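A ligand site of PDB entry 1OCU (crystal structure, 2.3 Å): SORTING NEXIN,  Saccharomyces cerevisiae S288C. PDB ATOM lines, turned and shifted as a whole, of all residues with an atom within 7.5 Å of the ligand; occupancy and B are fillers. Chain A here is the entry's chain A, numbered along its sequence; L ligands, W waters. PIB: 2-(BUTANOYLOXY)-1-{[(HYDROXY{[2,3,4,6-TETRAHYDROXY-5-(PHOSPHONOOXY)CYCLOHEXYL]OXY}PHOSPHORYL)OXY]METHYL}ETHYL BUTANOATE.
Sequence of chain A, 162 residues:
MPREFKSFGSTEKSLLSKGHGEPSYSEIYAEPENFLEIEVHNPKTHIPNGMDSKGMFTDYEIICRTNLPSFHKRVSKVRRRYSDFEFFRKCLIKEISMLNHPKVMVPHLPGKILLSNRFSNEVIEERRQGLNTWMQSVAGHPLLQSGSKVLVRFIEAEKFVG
Residues that only touch the ligand: Tyr 82. Hydrophobic or aromatic side chains that line the ligand: Tyr 82 and Ile 113. Eight residues have an atom within 4 Å of the ligand: Arg 81, Tyr 82, Ser 83, Glu 86, Lys 112, Ile 113, Arg 118 and Arg 127.
The side-chain carboxylate of Glu 86 sits at hydrogen-bond distance from an oxygen (O2) of the ligand, 2.7 Å away. An oxygen (O33) of the ligand is in hydrogen-bond range of the backbone NH of Ser 83 (3.1 Å). The side-chain hydroxyl (OG) of Ser 83 is in hydrogen-bond range of an oxygen (O33) of the ligand (2.7 Å). The side-chain amino group of Lys 112 lies within salt-bridge range of an oxygen (O11) of the ligand (2.7 Å). The backbone NH (N) of Ile 113 sits at hydrogen-bond distance from an oxygen (O5) of the ligand (2.8 Å). The backbone carbonyl oxygen (O) of Ile 113 lies within hydrogen-bond range of an oxygen (O5) of the ligand, 2.9 Å away. O4 of the ligand is in hydrogen-bond range of NH1 of Arg 127 (2.9 Å). O32 of the ligand is in salt-bridge range of NH2 of Arg 81 (3.1 Å). The guanidinium group of Arg 118 is in salt-bridge range of an oxygen (O32) of the ligand, 3.1 Å away.
The side-chain carboxylate (OE2) of Glu 86 is in salt-bridge range of the side-chain amino group (NZ) of Lys 112, at 3.0 Å. NH2 of Arg 127 sits at hydrogen-bond distance from O of Gly 111. The backbone NH (N) of Arg 81 is in hydrogen-bond range of the side-chain carboxylate (OD2) of Asp 84. The backbone NH of Gly 111 is in hydrogen-bond range of the side-chain hydroxyl of Tyr 82, at 2.9 Å.
Water W1 bridges the backbone NH (N) of Thr 58 (2.6 Å) and an oxygen (O31) of the ligand (2.8 Å).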
ATOM      1  N   GLY A  55      29.933 -15.329  17.426  1.00  0.00           N
ATOM      2  CA  GLY A  55      30.365 -15.209  16.036  1.00  0.00           C
ATOM      3  C   GLY A  55      30.585 -16.535  15.334  1.00  0.00           C
ATOM      4  O   GLY A  55      31.087 -16.570  14.209  1.00  0.00           O
ATOM      5  N   MET A  56      30.228 -17.633  16.009  1.00  0.00           N
ATOM      6  CA  MET A  56      30.378 -18.962  15.437  1.00  0.00           C
ATOM      7  C   MET A  56      29.743 -18.990  14.050  1.00  0.00           C
ATOM      8  O   MET A  56      28.630 -18.511  13.853  1.00  0.00           O
ATOM      9  CB  MET A  56      29.700 -19.996  16.348  1.00  0.00           C
ATOM     10  CG  MET A  56      29.762 -21.404  15.822  1.00  0.00           C
ATOM     11  SD  MET A  56      29.177 -22.616  17.013  1.00  0.00           S
ATOM     12  CE  MET A  56      27.592 -21.953  17.404  1.00  0.00           C
ATOM     13  N   PHE A  57      30.454 -19.564  13.070  1.00  0.00           N
ATOM     14  CA  PHE A  57      29.930 -19.591  11.713  1.00  0.00           C
ATOM     15  C   PHE A  57      30.506 -20.699  10.839  1.00  0.00           C
ATOM     16  O   PHE A  57      31.563 -21.260  11.138  1.00  0.00           O
ATOM     17  CB  PHE A  57      30.216 -18.234  11.042  1.00  0.00           C
ATOM     18  CG  PHE A  57      31.660 -18.049  10.637  1.00  0.00           C
ATOM     19  CD1 PHE A  57      32.103 -18.433   9.372  1.00  0.00           C
ATOM     20  CD2 PHE A  57      32.580 -17.478  11.515  1.00  0.00           C
ATOM     21  CE1 PHE A  57      33.432 -18.255   8.986  1.00  0.00           C
ATOM     22  CE2 PHE A  57      33.918 -17.292  11.147  1.00  0.00           C
ATOM     23  CZ  PHE A  57      34.348 -17.681   9.881  1.00  0.00           C
ATOM     24  N   THR A  58      29.798 -20.997   9.758  1.00  0.00           N
ATOM     25  CA  THR A  58      30.223 -22.020   8.815  1.00  0.00           C
ATOM     26  C   THR A  58      30.607 -21.383   7.476  1.00  0.00           C
ATOM     27  O   THR A  58      29.934 -20.470   7.001  1.00  0.00           O
ATOM     28  CB  THR A  58      29.097 -23.036   8.533  1.00  0.00           C
ATOM     29  OG1 THR A  58      28.623 -23.590   9.762  1.00  0.00           O
ATOM     30  CG2 THR A  58      29.607 -24.145   7.632  1.00  0.00           C
ATOM     31  N   ASP A  59      31.690 -21.856   6.876  1.00  0.00           N
ATOM     32  CA  ASP A  59      32.050 -21.350   5.553  1.00  0.00           C
ATOM     33  C   ASP A  59      32.316 -22.548   4.672  1.00  0.00           C
ATOM     34  O   ASP A  59      32.485 -23.661   5.157  1.00  0.00           O
ATOM     35  CB  ASP A  59      33.254 -20.378   5.614  1.00  0.00           C
ATOM     36  CG  ASP A  59      34.521 -21.003   6.116  1.00  0.00           C
ATOM     37  OD1 ASP A  59      35.471 -20.239   6.376  1.00  0.00           O
ATOM     38  OD2 ASP A  59      34.607 -22.251   6.249  1.00  0.00           O
ATOM     39  N   TYR A  60      32.321 -22.324   3.366  1.00  0.00           N
ATOM     40  CA  TYR A  60      32.520 -23.413   2.418  1.00  0.00           C
ATOM     41  C   TYR A  60      33.644 -23.090   1.462  1.00  0.00           C
ATOM     42  O   TYR A  60      33.949 -21.921   1.195  1.00  0.00           O
ATOM     43  CB  TYR A  60      31.229 -23.647   1.630  1.00  0.00           C
ATOM     44  CG  TYR A  60      30.004 -23.779   2.500  1.00  0.00           C
ATOM     45  CD1 TYR A  60      29.496 -22.685   3.193  1.00  0.00           C
ATOM     46  CD2 TYR A  60      29.394 -25.024   2.679  1.00  0.00           C
ATOM     47  CE1 TYR A  60      28.426 -22.820   4.067  1.00  0.00           C
ATOM     48  CE2 TYR A  60      28.317 -25.174   3.543  1.00  0.00           C
ATOM     49  CZ  TYR A  60      27.835 -24.068   4.239  1.00  0.00           C
ATOM     50  OH  TYR A  60      26.792 -24.218   5.134  1.00  0.00           O
ATOM     51  N   ARG A  80      34.010 -19.292   1.495  1.00  0.00           N
ATOM     52  CA  ARG A  80      32.965 -18.296   1.585  1.00  0.00           C
ATOM     53  C   ARG A  80      31.844 -18.699   2.540  1.00  0.00           C
ATOM     54  O   ARG A  80      31.496 -19.870   2.671  1.00  0.00           O
ATOM     55  CB  ARG A  80      32.368 -18.048   0.191  1.00  0.00           C
ATOM     56  CG  ARG A  80      33.355 -17.500  -0.853  1.00  0.00           C
ATOM     57  CD  ARG A  80      33.614 -16.023  -0.639  1.00  0.00           C
ATOM     58  NE  ARG A  80      34.354 -15.408  -1.733  1.00  0.00           N
ATOM     59  CZ  ARG A  80      35.679 -15.300  -1.810  1.00  0.00           C
ATOM     60  NH1 ARG A  80      36.441 -15.770  -0.840  1.00  0.00           N
ATOM     61  NH2 ARG A  80      36.232 -14.713  -2.860  1.00  0.00           N
ATOM     62  N   ARG A  81      31.294 -17.677   3.196  1.00  0.00           N
ATOM     63  CA  ARG A  81      30.184 -17.809   4.133  1.00  0.00           C
ATOM     64  C   ARG A  81      28.901 -17.691   3.328  1.00  0.00           C
ATOM     65  O   ARG A  81      28.895 -17.092   2.250  1.00  0.00           O
ATOM     66  CB  ARG A  81      30.165 -16.637   5.098  1.00  0.00           C
ATOM     67  CG  ARG A  81      30.967 -16.739   6.343  1.00  0.00           C
ATOM     68  CD  ARG A  81      30.183 -15.955   7.378  1.00  0.00           C
ATOM     69  NE  ARG A  81      31.015 -15.438   8.453  1.00  0.00           N
ATOM     70  CZ  ARG A  81      30.524 -14.893   9.559  1.00  0.00           C
ATOM     71  NH1 ARG A  81      31.364 -14.455  10.477  1.00  0.00           N
ATOM     72  NH2 ARG A  81      29.217 -14.825   9.748  1.00  0.00           N
ATOM     73  N   TYR A  82      27.800 -18.198   3.869  1.00  0.00           N
ATOM     74  CA  TYR A  82      26.523 -18.112   3.181  1.00  0.00           C
ATOM     75  C   TYR A  82      26.158 -16.649   2.942  1.00  0.00           C
ATOM     76  O   TYR A  82      25.673 -16.291   1.875  1.00  0.00           O
ATOM     77  CB  TYR A  82      25.420 -18.806   3.988  1.00  0.00           C
ATOM     78  CG  TYR A  82      24.064 -18.724   3.326  1.00  0.00           C
ATOM     79  CD1 TYR A  82      23.200 -17.662   3.586  1.00  0.00           C
ATOM     80  CD2 TYR A  82      23.654 -19.682   2.404  1.00  0.00           C
ATOM     81  CE1 TYR A  82      21.965 -17.560   2.940  1.00  0.00           C
ATOM     82  CE2 TYR A  82      22.425 -19.597   1.757  1.00  0.00           C
ATOM     83  CZ  TYR A  82      21.586 -18.537   2.023  1.00  0.00           C
ATOM     84  OH  TYR A  82      20.376 -18.436   1.359  1.00  0.00           O
ATOM     85  N   SER A  83      26.395 -15.797   3.932  1.00  0.00           N
ATOM     86  CA  SER A  83      26.083 -14.373   3.768  1.00  0.00           C
ATOM     87  C   SER A  83      26.995 -13.768   2.695  1.00  0.00           C
ATOM     88  O   SER A  83      26.656 -12.753   2.115  1.00  0.00           O
ATOM     89  CB  SER A  83      26.233 -13.617   5.090  1.00  0.00           C
ATOM     90  OG  SER A  83      27.541 -13.796   5.606  1.00  0.00           O
ATOM     91  N   ASP A  84      28.155 -14.376   2.478  1.00  0.00           N
ATOM     92  CA  ASP A  84      29.039 -13.873   1.420  1.00  0.00           C
ATOM     93  C   ASP A  84      28.289 -14.126   0.097  1.00  0.00           C
ATOM     94  O   ASP A  84      28.205 -13.233  -0.740  1.00  0.00           O
ATOM     95  CB  ASP A  84      30.379 -14.632   1.382  1.00  0.00           C
ATOM     96  CG  ASP A  84      31.335 -14.196   2.482  1.00  0.00           C
ATOM     97  OD1 ASP A  84      31.221 -13.060   2.981  1.00  0.00           O
ATOM     98  OD2 ASP A  84      32.234 -15.000   2.827  1.00  0.00           O
ATOM     99  N   PHE A  85      27.742 -15.323  -0.063  1.00  0.00           N
ATOM    100  CA  PHE A  85      26.964 -15.674  -1.263  1.00  0.00           C
ATOM    101  C   PHE A  85      25.789 -14.703  -1.401  1.00  0.00           C
ATOM    102  O   PHE A  85      25.486 -14.249  -2.508  1.00  0.00           O
ATOM    103  CB  PHE A  85      26.421 -17.103  -1.169  1.00  0.00           C
ATOM    104  CG  PHE A  85      27.457 -18.179  -1.347  1.00  0.00           C
ATOM    105  CD1 PHE A  85      27.678 -18.736  -2.600  1.00  0.00           C
ATOM    106  CD2 PHE A  85      28.191 -18.640  -0.259  1.00  0.00           C
ATOM    107  CE1 PHE A  85      28.623 -19.745  -2.769  1.00  0.00           C
ATOM    108  CE2 PHE A  85      29.140 -19.641  -0.423  1.00  0.00           C
ATOM    109  CZ  PHE A  85      29.360 -20.192  -1.684  1.00  0.00           C
ATOM    110  N   GLU A  86      25.122 -14.397  -0.296  1.00  0.00           N
ATOM    111  CA  GLU A  86      23.995 -13.465  -0.319  1.00  0.00           C
ATOM    112  C   GLU A  86      24.443 -12.090  -0.815  1.00  0.00           C
ATOM    113  O   GLU A  86      23.773 -11.446  -1.625  1.00  0.00           O
ATOM    114  CB  GLU A  86      23.384 -13.309   1.071  1.00  0.00           C
ATOM    115  CG  GLU A  86      22.567 -14.472   1.568  1.00  0.00           C
ATOM    116  CD  GLU A  86      21.931 -14.173   2.923  1.00  0.00           C
ATOM    117  OE1 GLU A  86      22.681 -14.000   3.907  1.00  0.00           O
ATOM    118  OE2 GLU A  86      20.674 -14.100   3.014  1.00  0.00           O
ATOM    119  N   GLY A 111      18.575 -20.603   0.680  1.00  0.00           N
ATOM    120  CA  GLY A 111      17.692 -20.058   1.713  1.00  0.00           C
ATOM    121  C   GLY A 111      18.239 -19.840   3.102  1.00  0.00           C
ATOM    122  O   GLY A 111      19.116 -20.576   3.572  1.00  0.00           O
ATOM    123  N   LYS A 112      17.720 -18.826   3.785  1.00  0.00           N
ATOM    124  CA  LYS A 112      18.129 -18.527   5.138  1.00  0.00           C
ATOM    125  C   LYS A 112      17.672 -19.668   6.059  1.00  0.00           C
ATOM    126  O   LYS A 112      16.708 -20.365   5.753  1.00  0.00           O
ATOM    127  CB  LYS A 112      17.511 -17.209   5.592  1.00  0.00           C
ATOM    128  CG  LYS A 112      18.122 -15.983   4.928  1.00  0.00           C
ATOM    129  CD  LYS A 112      17.377 -14.717   5.341  1.00  0.00           C
ATOM    130  CE  LYS A 112      18.050 -13.451   4.839  1.00  0.00           C
ATOM    131  NZ  LYS A 112      19.339 -13.198   5.526  1.00  0.00           N
ATOM    132  N   ILE A 113      18.370 -19.849   7.172  1.00  0.00           N
ATOM    133  CA  ILE A 113      18.042 -20.929   8.102  1.00  0.00           C
ATOM    134  C   ILE A 113      18.039 -20.515   9.571  1.00  0.00           C
ATOM    135  O   ILE A 113      18.781 -19.619   9.981  1.00  0.00           O
ATOM    136  CB  ILE A 113      19.037 -22.112   7.938  1.00  0.00           C
ATOM    137  CG1 ILE A 113      18.985 -22.648   6.512  1.00  0.00           C
ATOM    138  CG2 ILE A 113      18.726 -23.203   8.947  1.00  0.00           C
ATOM    139  CD1 ILE A 113      17.632 -23.178   6.098  1.00  0.00           C
ATOM    140  N   LEU A 114      17.207 -21.183  10.355  1.00  0.00           N
ATOM    141  CA  LEU A 114      17.066 -20.948  11.800  1.00  0.00           C
ATOM    142  C   LEU A 114      18.343 -21.311  12.564  1.00  0.00           C
ATOM    143  O   LEU A 114      18.872 -22.408  12.425  1.00  0.00           O
ATOM    144  CB  LEU A 114      15.871 -21.760  12.336  1.00  0.00           C
ATOM    145  CG  LEU A 114      15.371 -22.946  11.484  1.00  0.00           C
ATOM    146  CD1 LEU A 114      14.510 -23.859  12.336  1.00  0.00           C
ATOM    147  CD2 LEU A 114      14.575 -22.415  10.284  1.00  0.00           C
ATOM    148  N   LEU A 115      18.811 -20.371  13.394  1.00  0.00           N
ATOM    149  CA  LEU A 115      20.033 -20.540  14.184  1.00  0.00           C
ATOM    150  C   LEU A 115      20.386 -21.936  14.714  1.00  0.00           C
ATOM    151  O   LEU A 115      21.506 -22.408  14.537  1.00  0.00           O
ATOM    152  CB  LEU A 115      20.041 -19.548  15.348  1.00  0.00           C
ATOM    153  CG  LEU A 115      21.286 -19.533  16.256  1.00  0.00           C
ATOM    154  CD1 LEU A 115      22.536 -19.341  15.415  1.00  0.00           C
ATOM    155  CD2 LEU A 115      21.157 -18.433  17.290  1.00  0.00           C
ATOM    156  N   ARG A 118      20.859 -24.813  12.248  1.00  0.00           N
ATOM    157  CA  ARG A 118      21.781 -24.142  11.357  1.00  0.00           C
ATOM    158  C   ARG A 118      23.210 -24.698  11.399  1.00  0.00           C
ATOM    159  O   ARG A 118      23.943 -24.593  10.415  1.00  0.00           O
ATOM    160  CB  ARG A 118      21.769 -22.645  11.683  1.00  0.00           C
ATOM    161  CG  ARG A 118      22.916 -21.827  11.136  1.00  0.00           C
ATOM    162  CD  ARG A 118      22.726 -20.389  11.544  1.00  0.00           C
ATOM    163  NE  ARG A 118      23.967 -19.631  11.489  1.00  0.00           N
ATOM    164  CZ  ARG A 118      24.085 -18.342  11.789  1.00  0.00           C
ATOM    165  NH1 ARG A 118      23.008 -17.653  12.171  1.00  0.00           N
ATOM    166  NH2 ARG A 118      25.265 -17.740  11.699  1.00  0.00           N
ATOM    167  N   PHE A 119      23.593 -25.307  12.519  1.00  0.00           N
ATOM    168  CA  PHE A 119      24.936 -25.870  12.652  1.00  0.00           C
ATOM    169  C   PHE A 119      24.949 -27.396  12.706  1.00  0.00           C
ATOM    170  O   PHE A 119      25.984 -28.001  13.027  1.00  0.00           O
ATOM    171  CB  PHE A 119      25.632 -25.318  13.889  1.00  0.00           C
ATOM    172  CG  PHE A 119      26.024 -23.870  13.764  1.00  0.00           C
ATOM    173  CD1 PHE A 119      25.532 -22.930  14.667  1.00  0.00           C
ATOM    174  CD2 PHE A 119      26.870 -23.454  12.747  1.00  0.00           C
ATOM    175  CE1 PHE A 119      25.885 -21.575  14.553  1.00  0.00           C
ATOM    176  CE2 PHE A 119      27.223 -22.111  12.611  1.00  0.00           C
ATOM    177  CZ  PHE A 119      26.730 -21.171  13.514  1.00  0.00           C
ATOM    178  N   VAL A 123      21.893 -30.201   7.883  1.00  0.00           N
ATOM    179  CA  VAL A 123      21.624 -28.843   7.421  1.00  0.00           C
ATOM    180  C   VAL A 123      22.792 -28.256   6.644  1.00  0.00           C
ATOM    181  O   VAL A 123      22.601 -27.634   5.611  1.00  0.00           O
ATOM    182  CB  VAL A 123      21.273 -27.920   8.606  1.00  0.00           C
ATOM    183  CG1 VAL A 123      21.034 -26.498   8.126  1.00  0.00           C
ATOM    184  CG2 VAL A 123      20.034 -28.443   9.307  1.00  0.00           C
ATOM    185  N   ARG A 127      22.597 -27.425   2.522  1.00  0.00           N
ATOM    186  CA  ARG A 127      22.947 -26.079   2.102  1.00  0.00           C
ATOM    187  C   ARG A 127      24.162 -26.143   1.180  1.00  0.00           C
ATOM    188  O   ARG A 127      24.224 -25.438   0.185  1.00  0.00           O
ATOM    189  CB  ARG A 127      23.242 -25.213   3.312  1.00  0.00           C
ATOM    190  CG  ARG A 127      23.929 -23.905   2.986  1.00  0.00           C
ATOM    191  CD  ARG A 127      23.982 -23.010   4.180  1.00  0.00           C
ATOM    192  NE  ARG A 127      22.749 -22.252   4.351  1.00  0.00           N
ATOM    193  CZ  ARG A 127      22.573 -21.371   5.335  1.00  0.00           C
ATOM    194  NH1 ARG A 127      23.541 -21.171   6.216  1.00  0.00           N
ATOM    195  NH2 ARG A 127      21.448 -20.671   5.397  1.00  0.00           N
HETATM  196  C1  PIB L   1      21.319 -15.495   8.370  1.00  0.00           C
HETATM  197  C2  PIB L   1      22.692 -15.343   7.667  1.00  0.00           C
HETATM  198  C3  PIB L   1      23.594 -16.516   8.065  1.00  0.00           C
HETATM  199  C4  PIB L   1      22.905 -17.915   7.693  1.00  0.00           C
HETATM  200  C5  PIB L   1      21.553 -18.045   8.462  1.00  0.00           C
HETATM  201  C6  PIB L   1      20.633 -16.850   8.007  1.00  0.00           C
HETATM  202  O1  PIB L   1      20.505 -14.386   7.980  1.00  0.00           O
HETATM  203  O2  PIB L   1      22.502 -15.322   6.265  1.00  0.00           O
HETATM  204  O3  PIB L   1      24.832 -16.272   7.386  1.00  0.00           O
HETATM  205  O4  PIB L   1      23.751 -18.992   8.089  1.00  0.00           O
HETATM  206  O5  PIB L   1      20.932 -19.273   8.136  1.00  0.00           O
HETATM  207  O6  PIB L   1      19.385 -16.940   8.682  1.00  0.00           O
HETATM  208  P1  PIB L   1      20.187 -13.131   8.893  1.00  0.00           P
HETATM  209  O11 PIB L   1      19.755 -11.943   7.925  1.00  0.00           O
HETATM  210  O12 PIB L   1      21.444 -12.728   9.746  1.00  0.00           O
HETATM  211  O13 PIB L   1      18.949 -13.556   9.868  1.00  0.00           O
HETATM  212  P3  PIB L   1      26.265 -16.715   7.923  1.00  0.00           P
HETATM  213  O31 PIB L   1      26.342 -18.281   7.970  1.00  0.00           O
HETATM  214  O32 PIB L   1      26.444 -16.107   9.380  1.00  0.00           O
HETATM  215  O33 PIB L   1      27.324 -16.192   6.882  1.00  0.00           O
HETATM  216  C7  PIB L   1      19.134 -14.318  11.050  1.00  0.00           C
HETATM  217  C8  PIB L   1      17.969 -13.967  11.959  1.00  0.00           C
HETATM  218  O   HOH W   1      27.299 -20.213   9.828  1.00  0.00           O
HETATM  219  O   HOH W   2      25.766 -13.565   9.584  1.00  0.00           O
